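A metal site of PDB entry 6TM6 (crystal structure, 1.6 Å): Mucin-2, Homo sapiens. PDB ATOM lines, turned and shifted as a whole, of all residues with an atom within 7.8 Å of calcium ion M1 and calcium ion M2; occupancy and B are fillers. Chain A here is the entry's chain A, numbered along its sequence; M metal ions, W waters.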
ATOM      1  N   ILE A  10      24.532  -9.896  21.363  1.00  0.00           N
ATOM      2  CA  ILE A  10      23.379  -9.696  22.248  1.00  0.00           C
ATOM      3  C   ILE A  10      23.224  -8.195  22.489  1.00  0.00           C
ATOM      4  O   ILE A  10      24.180  -7.529  22.871  1.00  0.00           O
ATOM      5  CB  ILE A  10      23.554 -10.437  23.578  1.00  0.00           C
ATOM      6  CG1 ILE A  10      23.721 -11.944  23.334  1.00  0.00           C
ATOM      7  CG2 ILE A  10      22.393 -10.137  24.507  1.00  0.00           C
ATOM      8  CD1 ILE A  10      24.603 -12.635  24.362  1.00  0.00           C
ATOM      9  N   ASN A  11      22.014  -7.667  22.238  1.00  0.00           N
ATOM     10  CA  ASN A  11      21.767  -6.231  22.422  1.00  0.00           C
ATOM     11  C   ASN A  11      20.293  -6.060  22.788  1.00  0.00           C
ATOM     12  O   ASN A  11      19.459  -5.689  21.963  1.00  0.00           O
ATOM     13  CB  ASN A  11      22.139  -5.405  21.188  1.00  0.00           C
ATOM     14  CG  ASN A  11      21.993  -3.919  21.430  1.00  0.00           C
ATOM     15  OD1 ASN A  11      21.848  -3.494  22.564  1.00  0.00           O
ATOM     16  ND2 ASN A  11      22.041  -3.109  20.372  1.00  0.00           N
ATOM     17  N   GLU A  12      19.979  -6.341  24.051  1.00  0.00           N
ATOM     18  CA  GLU A  12      18.604  -6.353  24.532  1.00  0.00           C
ATOM     19  C   GLU A  12      18.222  -5.089  25.283  1.00  0.00           C
ATOM     20  O   GLU A  12      17.030  -4.798  25.409  1.00  0.00           O
ATOM     21  CB  GLU A  12      18.376  -7.553  25.443  1.00  0.00           C
ATOM     22  CG  GLU A  12      18.322  -8.870  24.696  1.00  0.00           C
ATOM     23  CD  GLU A  12      17.224  -8.876  23.643  1.00  0.00           C
ATOM     24  OE1 GLU A  12      16.036  -8.885  24.044  1.00  0.00           O
ATOM     25  OE2 GLU A  12      17.535  -8.855  22.431  1.00  0.00           O
ATOM     26  N   ASP A  13      19.200  -4.349  25.777  1.00  0.00           N
ATOM     27  CA  ASP A  13      18.986  -3.120  26.541  1.00  0.00           C
ATOM     28  C   ASP A  13      19.534  -1.961  25.724  1.00  0.00           C
ATOM     29  O   ASP A  13      20.311  -2.162  24.804  1.00  0.00           O
ATOM     30  CB  ASP A  13      19.689  -3.235  27.905  1.00  0.00           C
ATOM     31  CG  ASP A  13      19.303  -2.131  28.893  1.00  0.00           C
ATOM     32  OD1 ASP A  13      18.328  -1.389  28.678  1.00  0.00           O
ATOM     33  OD2 ASP A  13      20.011  -2.047  29.914  1.00  0.00           O
ATOM     34  N   HIS A  14      19.111  -0.743  26.067  1.00  0.00           N
ATOM     35  CA  HIS A  14      19.614   0.439  25.370  1.00  0.00           C
ATOM     36  C   HIS A  14      19.678   1.585  26.368  1.00  0.00           C
ATOM     37  O   HIS A  14      18.913   1.584  27.344  1.00  0.00           O
ATOM     38  CB  HIS A  14      18.743   0.829  24.170  1.00  0.00           C
ATOM     39  CG  HIS A  14      18.419  -0.334  23.284  1.00  0.00           C
ATOM     40  ND1 HIS A  14      19.291  -0.811  22.325  1.00  0.00           N
ATOM     41  CD2 HIS A  14      17.331  -1.135  23.224  1.00  0.00           C
ATOM     42  CE1 HIS A  14      18.748  -1.848  21.712  1.00  0.00           C
ATOM     43  NE2 HIS A  14      17.561  -2.069  22.235  1.00  0.00           N
ATOM     44  N   PRO A  15      20.564   2.563  26.159  1.00  0.00           N
ATOM     45  CA  PRO A  15      20.798   3.572  27.206  1.00  0.00           C
ATOM     46  C   PRO A  15      19.596   4.414  27.547  1.00  0.00           C
ATOM     47  O   PRO A  15      19.569   4.986  28.640  1.00  0.00           O
ATOM     48  CB  PRO A  15      21.922   4.434  26.621  1.00  0.00           C
ATOM     49  CG  PRO A  15      22.593   3.557  25.641  1.00  0.00           C
ATOM     50  CD  PRO A  15      21.507   2.720  25.043  1.00  0.00           C
ATOM     51  N   SER A  16      18.626   4.554  26.637  1.00  0.00           N
ATOM     52  CA  SER A  16      17.421   5.331  26.921  1.00  0.00           C
ATOM     53  C   SER A  16      16.166   4.465  26.929  1.00  0.00           C
ATOM     54  O   SER A  16      15.062   4.994  26.759  1.00  0.00           O
ATOM     55  CB  SER A  16      17.280   6.477  25.925  1.00  0.00           C
ATOM     56  OG  SER A  16      18.471   7.256  25.887  1.00  0.00           O
ATOM     57  N   SER A  17      16.309   3.154  27.104  1.00  0.00           N
ATOM     58  CA  SER A  17      15.201   2.220  27.206  1.00  0.00           C
ATOM     59  C   SER A  17      15.211   1.553  28.572  1.00  0.00           C
ATOM     60  O   SER A  17      16.262   1.441  29.213  1.00  0.00           O
ATOM     61  CB  SER A  17      15.265   1.135  26.126  1.00  0.00           C
ATOM     62  OG  SER A  17      15.524   1.720  24.874  1.00  0.00           O
ATOM     63  N   GLY A  18      14.040   1.066  28.991  1.00  0.00           N
ATOM     64  CA  GLY A  18      13.950   0.374  30.258  1.00  0.00           C
ATOM     65  C   GLY A  18      14.031   1.336  31.443  1.00  0.00           C
ATOM     66  O   GLY A  18      13.894   2.553  31.323  1.00  0.00           O
ATOM     67  N   SER A  19      14.299   0.745  32.603  1.00  0.00           N
ATOM     68  CA  SER A  19      14.241   1.457  33.867  1.00  0.00           C
ATOM     69  C   SER A  19      15.588   1.511  34.589  1.00  0.00           C
ATOM     70  O   SER A  19      15.632   1.948  35.753  1.00  0.00           O
ATOM     71  CB  SER A  19      13.214   0.810  34.791  1.00  0.00           C
ATOM     72  OG  SER A  19      13.571  -0.543  34.977  1.00  0.00           O
ATOM     73  N   ASP A  20      16.669   1.085  33.948  1.00  0.00           N
ATOM     74  CA  ASP A  20      17.953   0.980  34.640  1.00  0.00           C
ATOM     75  C   ASP A  20      18.873   2.180  34.444  1.00  0.00           C
ATOM     76  O   ASP A  20      19.954   2.197  35.034  1.00  0.00           O
ATOM     77  CB  ASP A  20      18.679  -0.294  34.214  1.00  0.00           C
ATOM     78  CG  ASP A  20      18.904  -0.411  32.706  1.00  0.00           C
ATOM     79  OD1 ASP A  20      18.291   0.325  31.895  1.00  0.00           O
ATOM     80  OD2 ASP A  20      19.712  -1.278  32.338  1.00  0.00           O
ATOM     81  N   ASP A  21      18.464   3.184  33.657  1.00  0.00           N
ATOM     82  CA  ASP A  21      19.298   4.363  33.403  1.00  0.00           C
ATOM     83  C   ASP A  21      20.722   3.954  33.003  1.00  0.00           C
ATOM     84  O   ASP A  21      21.720   4.352  33.615  1.00  0.00           O
ATOM     85  CB  ASP A  21      19.315   5.309  34.599  1.00  0.00           C
ATOM     86  CG  ASP A  21      20.000   6.631  34.276  1.00  0.00           C
ATOM     87  OD1 ASP A  21      19.790   7.138  33.158  1.00  0.00           O
ATOM     88  OD2 ASP A  21      20.785   7.129  35.117  1.00  0.00           O
ATOM     89  N   GLY A  22      20.802   3.136  31.962  1.00  0.00           N
ATOM     90  CA  GLY A  22      22.084   2.647  31.510  1.00  0.00           C
ATOM     91  C   GLY A  22      21.896   1.546  30.481  1.00  0.00           C
ATOM     92  O   GLY A  22      20.828   1.422  29.881  1.00  0.00           O
ATOM     93  N   ASP A  23      22.964   0.794  30.254  1.00  0.00           N
ATOM     94  CA  ASP A  23      22.935  -0.341  29.325  1.00  0.00           C
ATOM     95  C   ASP A  23      23.521  -1.551  30.018  1.00  0.00           C
ATOM     96  O   ASP A  23      24.701  -1.537  30.406  1.00  0.00           O
ATOM     97  CB  ASP A  23      23.711  -0.040  28.042  1.00  0.00           C
ATOM     98  CG  ASP A  23      23.346  -0.978  26.893  1.00  0.00           C
ATOM     99  OD1 ASP A  23      22.189  -1.424  26.816  1.00  0.00           O
ATOM    100  OD2 ASP A  23      24.203  -1.260  26.061  1.00  0.00           O
ATOM    101  N   ARG A  24      22.719  -2.604  30.172  1.00  0.00           N
ATOM    102  CA  ARG A  24      23.188  -3.865  30.725  1.00  0.00           C
ATOM    103  C   ARG A  24      22.879  -4.985  29.751  1.00  0.00           C
ATOM    104  O   ARG A  24      21.761  -5.079  29.238  1.00  0.00           O
ATOM    105  CB  ARG A  24      22.557  -4.136  32.084  1.00  0.00           C
ATOM    106  CG  ARG A  24      22.895  -3.025  33.063  1.00  0.00           C
ATOM    107  CD  ARG A  24      22.563  -3.330  34.514  1.00  0.00           C
ATOM    108  NE  ARG A  24      22.351  -2.076  35.237  1.00  0.00           N
ATOM    109  CZ  ARG A  24      22.448  -1.925  36.557  1.00  0.00           C
ATOM    110  NH1 ARG A  24      22.782  -2.941  37.334  1.00  0.00           N
ATOM    111  NH2 ARG A  24      22.231  -0.735  37.091  1.00  0.00           N
ATOM    112  N   GLU A  25      23.878  -5.814  29.485  1.00  0.00           N
ATOM    113  CA  GLU A  25      23.704  -6.981  28.636  1.00  0.00           C
ATOM    114  C   GLU A  25      24.134  -8.217  29.387  1.00  0.00           C
ATOM    115  O   GLU A  25      25.188  -8.224  30.047  1.00  0.00           O
ATOM    116  CB  GLU A  25      24.489  -6.863  27.330  1.00  0.00           C
ATOM    117  CG  GLU A  25      24.140  -5.612  26.512  1.00  0.00           C
ATOM    118  CD  GLU A  25      22.722  -5.613  25.993  1.00  0.00           C
ATOM    119  OE1 GLU A  25      22.075  -6.679  25.924  1.00  0.00           O
ATOM    120  OE2 GLU A  25      22.239  -4.521  25.630  1.00  0.00           O
ATOM    121  N   ARG A  40      31.152  -4.254  22.907  1.00  0.00           N
ATOM    122  CA  ARG A  40      31.455  -3.223  21.914  1.00  0.00           C
ATOM    123  C   ARG A  40      30.311  -2.232  21.790  1.00  0.00           C
ATOM    124  O   ARG A  40      29.136  -2.574  22.005  1.00  0.00           O
ATOM    125  CB  ARG A  40      31.733  -3.822  20.531  1.00  0.00           C
ATOM    126  CG  ARG A  40      32.960  -4.718  20.467  1.00  0.00           C
ATOM    127  CD  ARG A  40      34.221  -3.890  20.617  1.00  0.00           C
ATOM    128  NE  ARG A  40      35.384  -4.744  20.831  1.00  0.00           N
ATOM    129  CZ  ARG A  40      36.141  -5.236  19.848  1.00  0.00           C
ATOM    130  NH1 ARG A  40      35.876  -4.945  18.577  1.00  0.00           N
ATOM    131  NH2 ARG A  40      37.169  -6.027  20.146  1.00  0.00           N
ATOM    132  N   VAL A  42      27.668  -0.214  19.683  1.00  0.00           N
ATOM    133  CA  VAL A  42      26.919  -0.511  18.460  1.00  0.00           C
ATOM    134  C   VAL A  42      27.390   0.386  17.319  1.00  0.00           C
ATOM    135  O   VAL A  42      27.573  -0.077  16.188  1.00  0.00           O
ATOM    136  CB  VAL A  42      25.406  -0.358  18.720  1.00  0.00           C
ATOM    137  CG1 VAL A  42      24.621  -0.453  17.419  1.00  0.00           C
ATOM    138  CG2 VAL A  42      24.921  -1.413  19.734  1.00  0.00           C
ATOM    139  N   PHE A  64      27.763  -7.368  31.025  1.00  0.00           N
ATOM    140  CA  PHE A  64      28.104  -5.977  30.733  1.00  0.00           C
ATOM    141  C   PHE A  64      27.194  -5.015  31.493  1.00  0.00           C
ATOM    142  O   PHE A  64      25.977  -5.160  31.438  1.00  0.00           O
ATOM    143  CB  PHE A  64      28.015  -5.680  29.245  1.00  0.00           C
ATOM    144  CG  PHE A  64      28.303  -4.255  28.934  1.00  0.00           C
ATOM    145  CD1 PHE A  64      29.612  -3.817  28.860  1.00  0.00           C
ATOM    146  CD2 PHE A  64      27.268  -3.323  28.780  1.00  0.00           C
ATOM    147  CE1 PHE A  64      29.906  -2.499  28.600  1.00  0.00           C
ATOM    148  CE2 PHE A  64      27.559  -1.985  28.531  1.00  0.00           C
ATOM    149  CZ  PHE A  64      28.882  -1.574  28.443  1.00  0.00           C
ATOM    150  N   CYS A  66      26.767  -0.731  32.035  1.00  0.00           N
ATOM    151  CA  CYS A  66      27.107   0.692  31.913  1.00  0.00           C
ATOM    152  C   CYS A  66      26.014   1.490  32.612  1.00  0.00           C
ATOM    153  O   CYS A  66      24.825   1.267  32.366  1.00  0.00           O
ATOM    154  CB  CYS A  66      27.219   1.121  30.441  1.00  0.00           C
ATOM    155  SG  CYS A  66      27.723   2.866  30.211  1.00  0.00           S
ATOM    156  N   ASN A  68      24.510   5.279  33.245  1.00  0.00           N
ATOM    157  CA  ASN A  68      24.563   6.558  32.530  1.00  0.00           C
ATOM    158  C   ASN A  68      25.251   7.628  33.357  1.00  0.00           C
ATOM    159  O   ASN A  68      25.987   8.469  32.825  1.00  0.00           O
ATOM    160  CB  ASN A  68      23.157   7.015  32.134  1.00  0.00           C
ATOM    161  CG  ASN A  68      22.597   6.267  30.928  1.00  0.00           C
ATOM    162  OD1 ASN A  68      23.350   5.757  30.110  1.00  0.00           O
ATOM    163  ND2 ASN A  68      21.271   6.195  30.818  1.00  0.00           N
ATOM    164  N   TYR A  81      26.992   4.999  25.726  1.00  0.00           N
ATOM    165  CA  TYR A  81      26.746   4.485  24.381  1.00  0.00           C
ATOM    166  C   TYR A  81      25.846   3.250  24.481  1.00  0.00           C
ATOM    167  O   TYR A  81      25.700   2.638  25.541  1.00  0.00           O
ATOM    168  CB  TYR A  81      28.046   4.090  23.691  1.00  0.00           C
ATOM    169  CG  TYR A  81      29.060   5.186  23.528  1.00  0.00           C
ATOM    170  CD1 TYR A  81      28.680   6.479  23.168  1.00  0.00           C
ATOM    171  CD2 TYR A  81      30.410   4.935  23.706  1.00  0.00           C
ATOM    172  CE1 TYR A  81      29.625   7.482  23.004  1.00  0.00           C
ATOM    173  CE2 TYR A  81      31.355   5.924  23.539  1.00  0.00           C
ATOM    174  CZ  TYR A  81      30.954   7.199  23.196  1.00  0.00           C
ATOM    175  OH  TYR A  81      31.887   8.194  23.032  1.00  0.00           O
ATOM    176  N   ASP A  82      25.231   2.878  23.351  1.00  0.00           N
ATOM    177  CA  ASP A  82      24.561   1.586  23.314  1.00  0.00           C
ATOM    178  C   ASP A  82      25.594   0.501  23.022  1.00  0.00           C
ATOM    179  O   ASP A  82      26.372   0.606  22.068  1.00  0.00           O
ATOM    180  CB  ASP A  82      23.447   1.551  22.262  1.00  0.00           C
ATOM    181  CG  ASP A  82      22.552   0.321  22.399  1.00  0.00           C
ATOM    182  OD1 ASP A  82      22.548  -0.309  23.464  1.00  0.00           O
ATOM    183  OD2 ASP A  82      21.853  -0.016  21.428  1.00  0.00           O
ATOM    184  N   TYR A  83      25.615  -0.539  23.857  1.00  0.00           N
ATOM    185  CA  TYR A  83      26.580  -1.619  23.726  1.00  0.00           C
ATOM    186  C   TYR A  83      25.895  -2.917  23.353  1.00  0.00           C
ATOM    187  O   TYR A  83      24.701  -3.142  23.594  1.00  0.00           O
ATOM    188  CB  TYR A  83      27.347  -1.829  25.027  1.00  0.00           C
ATOM    189  CG  TYR A  83      28.289  -0.705  25.380  1.00  0.00           C
ATOM    190  CD1 TYR A  83      27.817   0.458  26.011  1.00  0.00           C
ATOM    191  CD2 TYR A  83      29.643  -0.811  25.113  1.00  0.00           C
ATOM    192  CE1 TYR A  83      28.692   1.501  26.342  1.00  0.00           C
ATOM    193  CE2 TYR A  83      30.517   0.219  25.441  1.00  0.00           C
ATOM    194  CZ  TYR A  83      30.034   1.373  26.047  1.00  0.00           C
ATOM    195  OH  TYR A  83      30.912   2.397  26.367  1.00  0.00           O
ATOM    196  N   LYS A  84      26.702  -3.799  22.778  1.00  0.00           N
ATOM    197  CA  LYS A  84      26.322  -5.170  22.450  1.00  0.00           C
ATOM    198  C   LYS A  84      27.467  -6.078  22.888  1.00  0.00           C
ATOM    199  O   LYS A  84      28.610  -5.636  23.014  1.00  0.00           O
ATOM    200  CB  LYS A  84      26.022  -5.312  20.952  1.00  0.00           C
ATOM    201  CG  LYS A  84      27.119  -4.729  20.051  1.00  0.00           C
ATOM    202  CD  LYS A  84      26.847  -4.946  18.567  1.00  0.00           C
ATOM    203  CE  LYS A  84      28.133  -4.715  17.755  1.00  0.00           C
ATOM    204  NZ  LYS A  84      27.859  -4.845  16.299  1.00  0.00           N
ATOM    205  N   ILE A  85      27.145  -7.347  23.128  1.00  0.00           N
ATOM    206  CA  ILE A  85      28.153  -8.285  23.609  1.00  0.00           C
ATOM    207  C   ILE A  85      28.089  -9.585  22.820  1.00  0.00           C
ATOM    208  O   ILE A  85      27.029 -10.016  22.347  1.00  0.00           O
ATOM    209  CB  ILE A  85      28.036  -8.594  25.124  1.00  0.00           C
ATOM    210  CG1 ILE A  85      26.768  -9.407  25.423  1.00  0.00           C
ATOM    211  CG2 ILE A  85      28.105  -7.316  25.943  1.00  0.00           C
ATOM    212  CD1 ILE A  85      26.737  -9.933  26.842  1.00  0.00           C
HETATM  213 CA    CA M   1      18.463   0.997  29.573  1.00  0.00          CA
HETATM  214 CA    CA M   2      22.610  -2.442  24.511  1.00  0.00          CA
HETATM  215  O   HOH W   1      18.278   3.255  30.352  1.00  0.00           O
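The side-chain carboxylate of Asp 13 is in hydrogen-bond range of the backbone NH of Arg 24 (2.8 Å).
OD2 of Asp 82 is in hydrogen-bond range of ND1 of His 14 (2.8 Å).
The backbone NH of His 14 lies close to the side-chain carboxylate of Asp 23 (3.2 Å).
The backbone carbonyl oxygen (O) of Asp 82 is in hydrogen-bond range of the backbone NH (N) of Val 42, at 2.8 Å.
The side-chain carboxylate (OE1) of Glu 25 lies within hydrogen-bond range of the backbone NH (N) of Glu 12 (2.8 Å).
O of Glu 25 sits at hydrogen-bond distance from N of Phe 64, 2.9 Å away.
The backbone NH of Gly 22 sits close to the side-chain amide nitrogen of Asn 68 (3.3 Å).
The backbone carbonyl oxygen of Asp 23 lies within hydrogen-bond range of the backbone NH of Cys 66.
Within 4 Å of calcium ion M1: Asp 13, His 14, Ser 17, Asp 20 and Gly 22.
Along chain A the residues within 4 Å of calcium ion M1 span positions 13 to 22.
Six residues have an atom within 4 Å of calcium ion M2: Asn 11, Asp 13, Asp 23, Glu 25, Asp 82 and Tyr 83.
The nearest printed residue that does not touch calcium ion M2 is His 14 (4.2 Å).
O of Ser 17 is bound to calcium ion M1 (2.3 Å).
Calcium ion M1 is bound by O of His 14 (2.3 Å).
Calcium ion M1 is bound by water W1 (2.4 Å).
O of Gly 22 binds calcium ion M1 (2.4 Å).
OD1 of Asp 20 is bound to calcium ion M1, at 2.4 Å.
OD1 of Asp 13 is bound to calcium ion M1, at 2.6 Å.
Calcium ion M1 has six donor atoms within binding distance.
Calcium ion M2 is bound by O of Asp 13 (2.3 Å), OD1 of Asn 11 (2.3 Å), OD1 of Asp 82 (2.4 Å), O of Tyr 83 (2.4 Å), OE2 of Glu 25 (2.4 Å), OD2 of Asp 23 (2.5 Å) and OD1 of Asp 23 (2.6 Å).
Water W1 lies within hydrogen-bond range of the backbone carbonyl oxygen of Pro 15 (2.8 Å), the backbone NH of Gly 22 (3.0 Å) and the backbone NH of Asp 21 (3.3 Å).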
